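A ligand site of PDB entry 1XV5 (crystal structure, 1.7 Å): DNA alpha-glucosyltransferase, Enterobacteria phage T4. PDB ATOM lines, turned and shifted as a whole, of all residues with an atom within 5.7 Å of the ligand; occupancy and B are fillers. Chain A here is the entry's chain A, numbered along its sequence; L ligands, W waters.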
ATOM      1  N   GLY A  14     -17.151   0.426  -7.140  1.00  0.00           N
ATOM      2  CA  GLY A  14     -16.259  -0.537  -6.516  1.00  0.00           C
ATOM      3  C   GLY A  14     -15.660  -0.144  -5.182  1.00  0.00           C
ATOM      4  O   GLY A  14     -14.769  -0.827  -4.664  1.00  0.00           O
ATOM      5  N   CME A  15     -16.128   0.956  -4.604  1.00  0.00           N
ATOM      6  CA  CME A  15     -15.628   1.385  -3.295  1.00  0.00           C
ATOM      7  CB  CME A  15     -15.041   2.790  -3.396  1.00  0.00           C
ATOM      8  SG  CME A  15     -13.429   2.788  -4.259  1.00  0.00           S
ATOM      9  SD  CME A  15     -13.851   3.444  -6.129  1.00  0.00           S
ATOM     10  CE  CME A  15     -12.782   4.918  -6.294  1.00  0.00           C
ATOM     11  CZ  CME A  15     -13.373   6.127  -5.601  1.00  0.00           C
ATOM     12  OH  CME A  15     -13.826   5.892  -4.429  1.00  0.00           O
ATOM     13  C   CME A  15     -16.719   1.297  -2.229  1.00  0.00           C
ATOM     14  O   CME A  15     -17.531   0.378  -2.253  1.00  0.00           O
ATOM     15  N   GLY A  16     -16.738   2.246  -1.304  1.00  0.00           N
ATOM     16  CA  GLY A  16     -17.700   2.228  -0.207  1.00  0.00           C
ATOM     17  C   GLY A  16     -19.181   2.170  -0.526  1.00  0.00           C
ATOM     18  O   GLY A  16     -19.953   1.516   0.186  1.00  0.00           O
ATOM     19  N   VAL A  17     -19.613   2.876  -1.561  1.00  0.00           N
ATOM     20  CA  VAL A  17     -21.013   2.866  -1.929  1.00  0.00           C
ATOM     21  C   VAL A  17     -21.401   1.482  -2.445  1.00  0.00           C
ATOM     22  O   VAL A  17     -22.484   0.968  -2.145  1.00  0.00           O
ATOM     23  CB  VAL A  17     -21.317   3.934  -2.994  1.00  0.00           C
ATOM     24  CG1 VAL A  17     -22.777   3.833  -3.441  1.00  0.00           C
ATOM     25  CG2 VAL A  17     -21.052   5.314  -2.416  1.00  0.00           C
ATOM     26  N   LYS A  19     -19.806  -1.317  -1.728  1.00  0.00           N
ATOM     27  CA  LYS A  19     -19.718  -2.190  -0.568  1.00  0.00           C
ATOM     28  C   LYS A  19     -20.992  -2.095   0.271  1.00  0.00           C
ATOM     29  O   LYS A  19     -21.575  -3.109   0.658  1.00  0.00           O
ATOM     30  CB  LYS A  19     -18.504  -1.797   0.287  1.00  0.00           C
ATOM     31  CG  LYS A  19     -18.337  -2.619   1.550  1.00  0.00           C
ATOM     32  CD  LYS A  19     -18.208  -4.099   1.243  1.00  0.00           C
ATOM     33  CE  LYS A  19     -17.859  -4.885   2.511  1.00  0.00           C
ATOM     34  NZ  LYS A  19     -17.866  -6.345   2.280  1.00  0.00           N
ATOM     35  N   ARG A  47     -12.575  -0.069 -10.549  1.00  0.00           N
ATOM     36  CA  ARG A  47     -12.727  -1.136  -9.559  1.00  0.00           C
ATOM     37  C   ARG A  47     -14.053  -1.892  -9.617  1.00  0.00           C
ATOM     38  O   ARG A  47     -14.516  -2.404  -8.598  1.00  0.00           O
ATOM     39  CB  ARG A  47     -12.547  -0.558  -8.157  1.00  0.00           C
ATOM     40  CG  ARG A  47     -11.345   0.375  -8.015  1.00  0.00           C
ATOM     41  CD  ARG A  47     -11.222   0.907  -6.591  1.00  0.00           C
ATOM     42  NE  ARG A  47     -10.508   2.186  -6.570  1.00  0.00           N
ATOM     43  CZ  ARG A  47      -9.291   2.372  -6.067  1.00  0.00           C
ATOM     44  NH1 ARG A  47      -8.617   1.358  -5.526  1.00  0.00           N
ATOM     45  NH2 ARG A  47      -8.737   3.580  -6.103  1.00  0.00           N
ATOM     46  N   SER A  50     -13.752  -5.199  -7.911  1.00  0.00           N
ATOM     47  CA  SER A  50     -13.246  -5.304  -6.546  1.00  0.00           C
ATOM     48  C   SER A  50     -14.164  -6.110  -5.629  1.00  0.00           C
ATOM     49  O   SER A  50     -13.677  -6.842  -4.760  1.00  0.00           O
ATOM     50  CB  SER A  50     -13.026  -3.901  -5.963  1.00  0.00           C
ATOM     51  OG  SER A  50     -11.952  -3.260  -6.622  1.00  0.00           O
ATOM     52  N   HIS A  51     -15.471  -5.985  -5.825  1.00  0.00           N
ATOM     53  CA  HIS A  51     -16.422  -6.720  -4.996  1.00  0.00           C
ATOM     54  C   HIS A  51     -17.213  -7.697  -5.852  1.00  0.00           C
ATOM     55  O   HIS A  51     -17.433  -7.455  -7.036  1.00  0.00           O
ATOM     56  CB  HIS A  51     -17.386  -5.760  -4.289  1.00  0.00           C
ATOM     57  CG  HIS A  51     -16.698  -4.775  -3.393  1.00  0.00           C
ATOM     58  ND1 HIS A  51     -16.252  -3.549  -3.835  1.00  0.00           N
ATOM     59  CD2 HIS A  51     -16.379  -4.844  -2.076  1.00  0.00           C
ATOM     60  CE1 HIS A  51     -15.683  -2.904  -2.829  1.00  0.00           C
ATOM     61  NE2 HIS A  51     -15.746  -3.668  -1.761  1.00  0.00           N
ATOM     62  N   ILE A 203      -4.576   0.074   3.819  1.00  0.00           N
ATOM     63  CA  ILE A 203      -5.556  -0.088   2.732  1.00  0.00           C
ATOM     64  C   ILE A 203      -6.388   1.177   2.580  1.00  0.00           C
ATOM     65  O   ILE A 203      -6.730   1.838   3.569  1.00  0.00           O
ATOM     66  CB  ILE A 203      -6.511  -1.290   2.962  1.00  0.00           C
ATOM     67  CG1 ILE A 203      -7.139  -1.225   4.357  1.00  0.00           C
ATOM     68  CG2 ILE A 203      -5.752  -2.604   2.750  1.00  0.00           C
ATOM     69  CD1 ILE A 203      -8.276  -2.237   4.569  1.00  0.00           C
ATOM     70  N   GLY A 204      -6.722   1.503   1.339  1.00  0.00           N
ATOM     71  CA  GLY A 204      -7.530   2.690   1.057  1.00  0.00           C
ATOM     72  C   GLY A 204      -7.446   3.056  -0.415  1.00  0.00           C
ATOM     73  O   GLY A 204      -7.461   2.179  -1.276  1.00  0.00           O
ATOM     74  N   ARG A 205      -7.379   4.355  -0.692  1.00  0.00           N
ATOM     75  CA  ARG A 205      -7.254   4.843  -2.068  1.00  0.00           C
ATOM     76  C   ARG A 205      -6.498   6.163  -2.052  1.00  0.00           C
ATOM     77  O   ARG A 205      -6.230   6.703  -0.987  1.00  0.00           O
ATOM     78  CB  ARG A 205      -8.634   5.002  -2.725  1.00  0.00           C
ATOM     79  CG  ARG A 205      -9.661   5.774  -1.936  1.00  0.00           C
ATOM     80  CD  ARG A 205     -11.033   5.592  -2.580  1.00  0.00           C
ATOM     81  NE  ARG A 205     -12.087   6.268  -1.830  1.00  0.00           N
ATOM     82  CZ  ARG A 205     -12.300   7.582  -1.854  1.00  0.00           C
ATOM     83  NH1 ARG A 205     -13.284   8.103  -1.127  1.00  0.00           N
ATOM     84  NH2 ARG A 205     -11.538   8.375  -2.594  1.00  0.00           N
ATOM     85  N   TRP A 209      -7.026  12.571   2.641  1.00  0.00           N
ATOM     86  CA  TRP A 209      -7.612  12.387   3.973  1.00  0.00           C
ATOM     87  C   TRP A 209      -7.627  10.932   4.412  1.00  0.00           C
ATOM     88  O   TRP A 209      -8.003  10.620   5.548  1.00  0.00           O
ATOM     89  CB  TRP A 209      -9.013  12.996   4.095  1.00  0.00           C
ATOM     90  CG  TRP A 209     -10.089  12.519   3.165  1.00  0.00           C
ATOM     91  CD1 TRP A 209     -10.514  13.136   2.023  1.00  0.00           C
ATOM     92  CD2 TRP A 209     -10.964  11.396   3.361  1.00  0.00           C
ATOM     93  NE1 TRP A 209     -11.608  12.474   1.502  1.00  0.00           N
ATOM     94  CE2 TRP A 209     -11.902  11.407   2.307  1.00  0.00           C
ATOM     95  CE3 TRP A 209     -11.046  10.382   4.330  1.00  0.00           C
ATOM     96  CZ2 TRP A 209     -12.910  10.442   2.190  1.00  0.00           C
ATOM     97  CZ3 TRP A 209     -12.058   9.424   4.217  1.00  0.00           C
ATOM     98  CH2 TRP A 209     -12.974   9.468   3.151  1.00  0.00           C
ATOM     99  N   LYS A 210      -7.192  10.029   3.529  1.00  0.00           N
ATOM    100  CA  LYS A 210      -7.140   8.611   3.861  1.00  0.00           C
ATOM    101  C   LYS A 210      -5.842   8.352   4.631  1.00  0.00           C
ATOM    102  O   LYS A 210      -5.616   7.250   5.124  1.00  0.00           O
ATOM    103  CB  LYS A 210      -7.165   7.749   2.588  1.00  0.00           C
ATOM    104  CG  LYS A 210      -8.483   7.804   1.838  1.00  0.00           C
ATOM    105  CD  LYS A 210      -9.608   7.057   2.561  1.00  0.00           C
ATOM    106  CE  LYS A 210     -10.876   7.059   1.728  1.00  0.00           C
ATOM    107  NZ  LYS A 210     -12.018   6.309   2.350  1.00  0.00           N
ATOM    108  N   GLU A 233      -2.180  -0.921  -0.151  1.00  0.00           N
ATOM    109  CA  GLU A 233      -3.059  -1.390  -1.212  1.00  0.00           C
ATOM    110  C   GLU A 233      -4.182  -0.427  -1.575  1.00  0.00           C
ATOM    111  O   GLU A 233      -4.803   0.167  -0.704  1.00  0.00           O
ATOM    112  CB  GLU A 233      -3.673  -2.730  -0.829  1.00  0.00           C
ATOM    113  CG  GLU A 233      -2.691  -3.875  -0.626  1.00  0.00           C
ATOM    114  CD  GLU A 233      -3.391  -5.227  -0.462  1.00  0.00           C
ATOM    115  OE1 GLU A 233      -4.450  -5.410  -1.082  1.00  0.00           O
ATOM    116  OE2 GLU A 233      -2.869  -6.097   0.256  1.00  0.00           O
ATOM    117  N   GLY A 234      -4.436  -0.303  -2.879  1.00  0.00           N
ATOM    118  CA  GLY A 234      -5.522   0.542  -3.337  1.00  0.00           C
ATOM    119  C   GLY A 234      -5.185   1.919  -3.878  1.00  0.00           C
ATOM    120  O   GLY A 234      -6.091   2.648  -4.291  1.00  0.00           O
ATOM    121  N   ASP A 274      -1.849  -1.084  -6.850  1.00  0.00           N
ATOM    122  CA  ASP A 274      -2.740  -0.097  -7.447  1.00  0.00           C
ATOM    123  C   ASP A 274      -4.217  -0.238  -7.179  1.00  0.00           C
ATOM    124  O   ASP A 274      -4.936   0.746  -7.049  1.00  0.00           O
ATOM    125  CB  ASP A 274      -2.517  -0.026  -8.967  1.00  0.00           C
ATOM    126  CG  ASP A 274      -2.964  -1.293  -9.694  1.00  0.00           C
ATOM    127  OD1 ASP A 274      -3.107  -1.231 -10.938  1.00  0.00           O
ATOM    128  OD2 ASP A 274      -3.169  -2.330  -9.053  1.00  0.00           O
ATOM    129  N   CME A 275      -4.674  -1.480  -7.099  1.00  0.00           N
ATOM    130  CA  CME A 275      -6.088  -1.759  -6.907  1.00  0.00           C
ATOM    131  CB  CME A 275      -6.780  -1.697  -8.272  1.00  0.00           C
ATOM    132  SG  CME A 275      -8.545  -2.122  -8.309  1.00  0.00           S
ATOM    133  SD  CME A 275      -8.547  -4.160  -8.344  1.00  0.00           S
ATOM    134  CE  CME A 275      -8.064  -4.565 -10.052  1.00  0.00           C
ATOM    135  CZ  CME A 275      -9.152  -5.320 -10.784  1.00  0.00           C
ATOM    136  OH  CME A 275     -10.044  -4.573 -11.303  1.00  0.00           O
ATOM    137  C   CME A 275      -6.178  -3.163  -6.342  1.00  0.00           C
ATOM    138  O   CME A 275      -5.308  -3.996  -6.605  1.00  0.00           O
ATOM    139  N   TYR A 276      -7.206  -3.444  -5.546  1.00  0.00           N
ATOM    140  CA  TYR A 276      -7.320  -4.786  -5.002  1.00  0.00           C
ATOM    141  C   TYR A 276      -8.710  -5.367  -5.045  1.00  0.00           C
ATOM    142  O   TYR A 276      -9.716  -4.646  -5.013  1.00  0.00           O
ATOM    143  CB  TYR A 276      -6.777  -4.835  -3.562  1.00  0.00           C
ATOM    144  CG  TYR A 276      -7.513  -3.986  -2.532  1.00  0.00           C
ATOM    145  CD1 TYR A 276      -8.661  -4.461  -1.875  1.00  0.00           C
ATOM    146  CD2 TYR A 276      -7.018  -2.742  -2.158  1.00  0.00           C
ATOM    147  CE1 TYR A 276      -9.285  -3.711  -0.874  1.00  0.00           C
ATOM    148  CE2 TYR A 276      -7.639  -1.979  -1.176  1.00  0.00           C
ATOM    149  CZ  TYR A 276      -8.766  -2.464  -0.527  1.00  0.00           C
ATOM    150  OH  TYR A 276      -9.356  -1.716   0.466  1.00  0.00           O
ATOM    151  N   ILE A 277      -8.745  -6.685  -5.148  1.00  0.00           N
ATOM    152  CA  ILE A 277      -9.992  -7.430  -5.146  1.00  0.00           C
ATOM    153  C   ILE A 277     -10.211  -7.582  -3.641  1.00  0.00           C
ATOM    154  O   ILE A 277      -9.335  -8.066  -2.924  1.00  0.00           O
ATOM    155  CB  ILE A 277      -9.822  -8.818  -5.791  1.00  0.00           C
ATOM    156  CG1 ILE A 277      -9.423  -8.648  -7.260  1.00  0.00           C
ATOM    157  CG2 ILE A 277     -11.126  -9.606  -5.662  1.00  0.00           C
ATOM    158  CD1 ILE A 277     -10.390  -7.809  -8.077  1.00  0.00           C
ATOM    159  N   ASN A 278     -11.370  -7.144  -3.164  1.00  0.00           N
ATOM    160  CA  ASN A 278     -11.675  -7.172  -1.735  1.00  0.00           C
ATOM    161  C   ASN A 278     -11.343  -8.491  -1.032  1.00  0.00           C
ATOM    162  O   ASN A 278     -10.616  -8.478  -0.028  1.00  0.00           O
ATOM    163  CB  ASN A 278     -13.154  -6.814  -1.526  1.00  0.00           C
ATOM    164  CG  ASN A 278     -13.466  -6.492  -0.082  1.00  0.00           C
ATOM    165  OD1 ASN A 278     -13.994  -7.330   0.655  1.00  0.00           O
ATOM    166  ND2 ASN A 278     -13.125  -5.279   0.348  1.00  0.00           N
ATOM    167  N   MET A 281      -7.594  -9.061  -0.722  1.00  0.00           N
ATOM    168  CA  MET A 281      -6.973  -8.185   0.271  1.00  0.00           C
ATOM    169  C   MET A 281      -7.246  -8.743   1.667  1.00  0.00           C
ATOM    170  O   MET A 281      -6.344  -8.797   2.493  1.00  0.00           O
ATOM    171  CB  MET A 281      -7.542  -6.769   0.144  1.00  0.00           C
ATOM    172  CG  MET A 281      -7.018  -5.779   1.179  1.00  0.00           C
ATOM    173  SD  MET A 281      -7.806  -5.932   2.812  1.00  0.00           S
ATOM    174  CE  MET A 281      -9.408  -5.173   2.457  1.00  0.00           C
ATOM    175  N   GLN A 293      -5.383   2.051   8.893  1.00  0.00           N
ATOM    176  CA  GLN A 293      -6.480   2.795   8.287  1.00  0.00           C
ATOM    177  C   GLN A 293      -6.305   4.139   8.970  1.00  0.00           C
ATOM    178  O   GLN A 293      -6.702   4.321  10.127  1.00  0.00           O
ATOM    179  CB  GLN A 293      -7.823   2.161   8.646  1.00  0.00           C
ATOM    180  CG  GLN A 293      -8.896   2.404   7.594  1.00  0.00           C
ATOM    181  CD  GLN A 293      -9.441   3.820   7.621  1.00  0.00           C
ATOM    182  OE1 GLN A 293      -8.828   4.724   8.184  1.00  0.00           O
ATOM    183  NE2 GLN A 293     -10.605   4.020   7.018  1.00  0.00           N
ATOM    184  N   GLU A 307     -15.301   3.606   8.588  1.00  0.00           N
ATOM    185  CA  GLU A 307     -15.376   3.250   7.174  1.00  0.00           C
ATOM    186  C   GLU A 307     -15.220   1.749   7.018  1.00  0.00           C
ATOM    187  O   GLU A 307     -14.826   1.048   7.944  1.00  0.00           O
ATOM    188  CB  GLU A 307     -14.287   3.979   6.402  1.00  0.00           C
ATOM    189  CG  GLU A 307     -14.438   5.479   6.477  1.00  0.00           C
ATOM    190  CD  GLU A 307     -13.323   6.213   5.765  1.00  0.00           C
ATOM    191  OE1 GLU A 307     -12.236   6.378   6.356  1.00  0.00           O
ATOM    192  OE2 GLU A 307     -13.541   6.600   4.601  1.00  0.00           O
ATOM    193  N   TYR A 308     -15.539   1.240   5.827  1.00  0.00           N
ATOM    194  CA  TYR A 308     -15.401  -0.189   5.597  1.00  0.00           C
ATOM    195  C   TYR A 308     -13.995  -0.707   5.811  1.00  0.00           C
ATOM    196  O   TYR A 308     -13.815  -1.779   6.383  1.00  0.00           O
ATOM    197  CB  TYR A 308     -15.923  -0.555   4.204  1.00  0.00           C
ATOM    198  CG  TYR A 308     -17.428  -0.598   4.167  1.00  0.00           C
ATOM    199  CD1 TYR A 308     -18.168   0.344   3.463  1.00  0.00           C
ATOM    200  CD2 TYR A 308     -18.126  -1.557   4.920  1.00  0.00           C
ATOM    201  CE1 TYR A 308     -19.563   0.341   3.510  1.00  0.00           C
ATOM    202  CE2 TYR A 308     -19.513  -1.559   4.974  1.00  0.00           C
ATOM    203  CZ  TYR A 308     -20.223  -0.611   4.267  1.00  0.00           C
ATOM    204  OH  TYR A 308     -21.602  -0.603   4.356  1.00  0.00           O
ATOM    205  N   THR A 309     -12.987   0.046   5.383  1.00  0.00           N
ATOM    206  CA  THR A 309     -11.625  -0.421   5.599  1.00  0.00           C
ATOM    207  C   THR A 309     -11.318  -0.529   7.082  1.00  0.00           C
ATOM    208  O   THR A 309     -10.509  -1.362   7.490  1.00  0.00           O
ATOM    209  CB  THR A 309     -10.574   0.488   4.902  1.00  0.00           C
ATOM    210  OG1 THR A 309     -10.852   1.859   5.204  1.00  0.00           O
ATOM    211  CG2 THR A 309     -10.610   0.278   3.390  1.00  0.00           C
ATOM    212  N   HIS A 310     -11.966   0.297   7.909  1.00  0.00           N
ATOM    213  CA  HIS A 310     -11.765   0.224   9.359  1.00  0.00           C
ATOM    214  C   HIS A 310     -12.290  -1.139   9.824  1.00  0.00           C
ATOM    215  O   HIS A 310     -11.606  -1.905  10.503  1.00  0.00           O
ATOM    216  CB  HIS A 310     -12.591   1.282  10.099  1.00  0.00           C
ATOM    217  CG  HIS A 310     -12.002   2.662  10.090  1.00  0.00           C
ATOM    218  ND1 HIS A 310     -12.696   3.748   9.627  1.00  0.00           N
ATOM    219  CD2 HIS A 310     -10.827   3.132  10.576  1.00  0.00           C
ATOM    220  CE1 HIS A 310     -11.987   4.840   9.831  1.00  0.00           C
ATOM    221  NE2 HIS A 310     -10.850   4.496  10.411  1.00  0.00           N
ATOM    222  N   GLU A 312     -12.980  -3.834   8.133  1.00  0.00           N
ATOM    223  CA  GLU A 312     -12.309  -4.978   7.542  1.00  0.00           C
ATOM    224  C   GLU A 312     -11.069  -5.382   8.327  1.00  0.00           C
ATOM    225  O   GLU A 312     -10.769  -6.569   8.440  1.00  0.00           O
ATOM    226  CB  GLU A 312     -11.985  -4.670   6.074  1.00  0.00           C
ATOM    227  CG  GLU A 312     -13.254  -4.678   5.212  1.00  0.00           C
ATOM    228  CD  GLU A 312     -13.077  -4.035   3.844  1.00  0.00           C
ATOM    229  OE1 GLU A 312     -13.957  -4.284   2.982  1.00  0.00           O
ATOM    230  OE2 GLU A 312     -12.110  -3.287   3.628  1.00  0.00           O
HETATM  231  N1  LIG L   1     -11.862  -1.513  -1.820  1.00  0.00           N
HETATM  232  C1  LIG L   1     -11.566  -2.582  -2.643  1.00  0.00           C
HETATM  233  N2  LIG L   1     -10.545  -2.353  -3.533  1.00  0.00           N
HETATM  234  C2  LIG L   1      -9.803  -1.198  -3.671  1.00  0.00           C
HETATM  235  C3  LIG L   1     -10.159  -0.147  -2.766  1.00  0.00           C
HETATM  236  C4  LIG L   1     -11.152  -0.336  -1.894  1.00  0.00           C
HETATM  237  O1  LIG L   1     -12.160  -3.643  -2.585  1.00  0.00           O
HETATM  238  O2  LIG L   1      -8.907  -1.145  -4.516  1.00  0.00           O
HETATM  239  C5  LIG L   1     -12.959  -1.682  -0.863  1.00  0.00           C
HETATM  240  C6  LIG L   1     -12.565  -1.518   0.596  1.00  0.00           C
HETATM  241  O3  LIG L   1     -11.980  -2.704   1.098  1.00  0.00           O
HETATM  242  C7  LIG L   1     -13.918  -1.181   1.208  1.00  0.00           C
HETATM  243  C8  LIG L   1     -14.499  -0.243   0.160  1.00  0.00           C
HETATM  244  O4  LIG L   1     -13.902  -0.649  -1.102  1.00  0.00           O
HETATM  245  O5  LIG L   1     -14.704  -2.368   1.292  1.00  0.00           O
HETATM  246  C9  LIG L   1     -14.224   1.229   0.391  1.00  0.00           C
HETATM  247  O6  LIG L   1     -15.096   1.738   1.384  1.00  0.00           O
HETATM  248  P1  LIG L   1     -14.610   2.696   2.570  1.00  0.00           P
HETATM  249  O7  LIG L   1     -15.818   2.983   3.367  1.00  0.00           O
HETATM  250  O8  LIG L   1     -13.430   2.074   3.225  1.00  0.00           O
HETATM  251  O9  LIG L   1     -14.087   4.060   1.835  1.00  0.00           O
HETATM  252  P2  LIG L   1     -14.577   4.834   0.471  1.00  0.00           P
HETATM  253  O10 LIG L   1     -14.416   6.291   0.726  1.00  0.00           O
HETATM  254  O11 LIG L   1     -13.871   4.215  -0.675  1.00  0.00           O
HETATM  255  O12 LIG L   1     -16.131   4.501   0.371  1.00  0.00           O
HETATM  256  O   HOH W   1     -16.238   8.101   1.455  1.00  0.00           O
HETATM  257  O   HOH W   2     -11.379   2.906  -0.383  1.00  0.00           O
HETATM  258  O   HOH W   3     -11.083   3.563   2.526  1.00  0.00           O
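The side-chain carboxylate (OE1) of Glu 307 lies within hydrogen-bond range of the side-chain amide nitrogen (NE2) of Gln 293, at 2.9 Å. O of Ser 50 is in hydrogen-bond range of N of Asn 278, 2.8 Å away. The side-chain hydroxyl of Ser 50 sits at hydrogen-bond distance from the backbone carbonyl oxygen of Tyr 276. The backbone carbonyl oxygen (O) of Arg 47 lies close to the side-chain hydroxyl (OG) of Ser 50. N of Gly 204 is in hydrogen-bond range of O of Glu 233 (3.1 Å). The guanidinium group of Arg 205 is in hydrogen-bond range of OH of CME 15 (3.1 Å). OE1 of Glu 312 is in hydrogen-bond range of ND2 of Asn 278. SD of CME 15 lies close to the guanidinium group (NE) of Arg 47.
Water W3 lies within hydrogen-bond range of an oxygen (O8) of the ligand (2.9 Å), the side-chain amino group of Lys 210 (2.9 Å) and the side-chain hydroxyl of Thr 309 (3.2 Å).
Gly 14 touches the ligand. CME 15 touches the ligand (CB to O11, 3.3 Å). Lys 19 touches the ligand. Ser 50 touches the ligand. Gly 204 touches the ligand (O to C3, 3.9 Å). CA of Gly 234 touches O2 of the ligand, 3.96 Å away. CME 275 touches the ligand (CA to O2, 3.7 Å). CE of Met 281 touches O3 of the ligand, at 3.8 Å. Glu 307 touches the ligand. Hydrophobic or aromatic side chains that line the ligand: His 51, Tyr 276, Met 281 and Tyr 308. The nearest printed residue that does not touch the ligand is Trp 209 (4.2 Å).
An oxygen (O5) of the ligand lies within hydrogen-bond range of a ring nitrogen (NE2) of His 51 (3.5 Å). OG1 of Thr 309 sits at hydrogen-bond distance from O8 of the ligand (3.3 Å). The side-chain hydroxyl (OH) of Tyr 276 lies within hydrogen-bond range of an oxygen (O3) of the ligand (2.9 Å). O2 of the ligand is in hydrogen-bond range of N of Tyr 276 (3.0 Å). The backbone NH of Gly 16 sits close to an oxygen (O12) of the ligand (2.9 Å). NZ of Lys 210 lies within salt-bridge range of O10 of the ligand, at 2.9 Å. A nitrogen (N2) of the ligand sits at hydrogen-bond distance from the backbone carbonyl oxygen (O) of Tyr 276 (2.9 Å). The backbone NH (N) of Tyr 308 lies within hydrogen-bond range of an oxygen (O7) of the ligand, 3.0 Å away. O2 of the ligand is in hydrogen-bond range of NH1 of Arg 47. NH1 of Arg 205 lies within salt-bridge range of O10 of the ligand. O8 of the ligand is in hydrogen-bond range of N of Thr 309, 3.0 Å away. ND2 of Asn 278 sits at hydrogen-bond distance from O3 of the ligand. OE2 of Glu 312 sits at hydrogen-bond distance from O3 of the ligand, at 2.6 Å.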
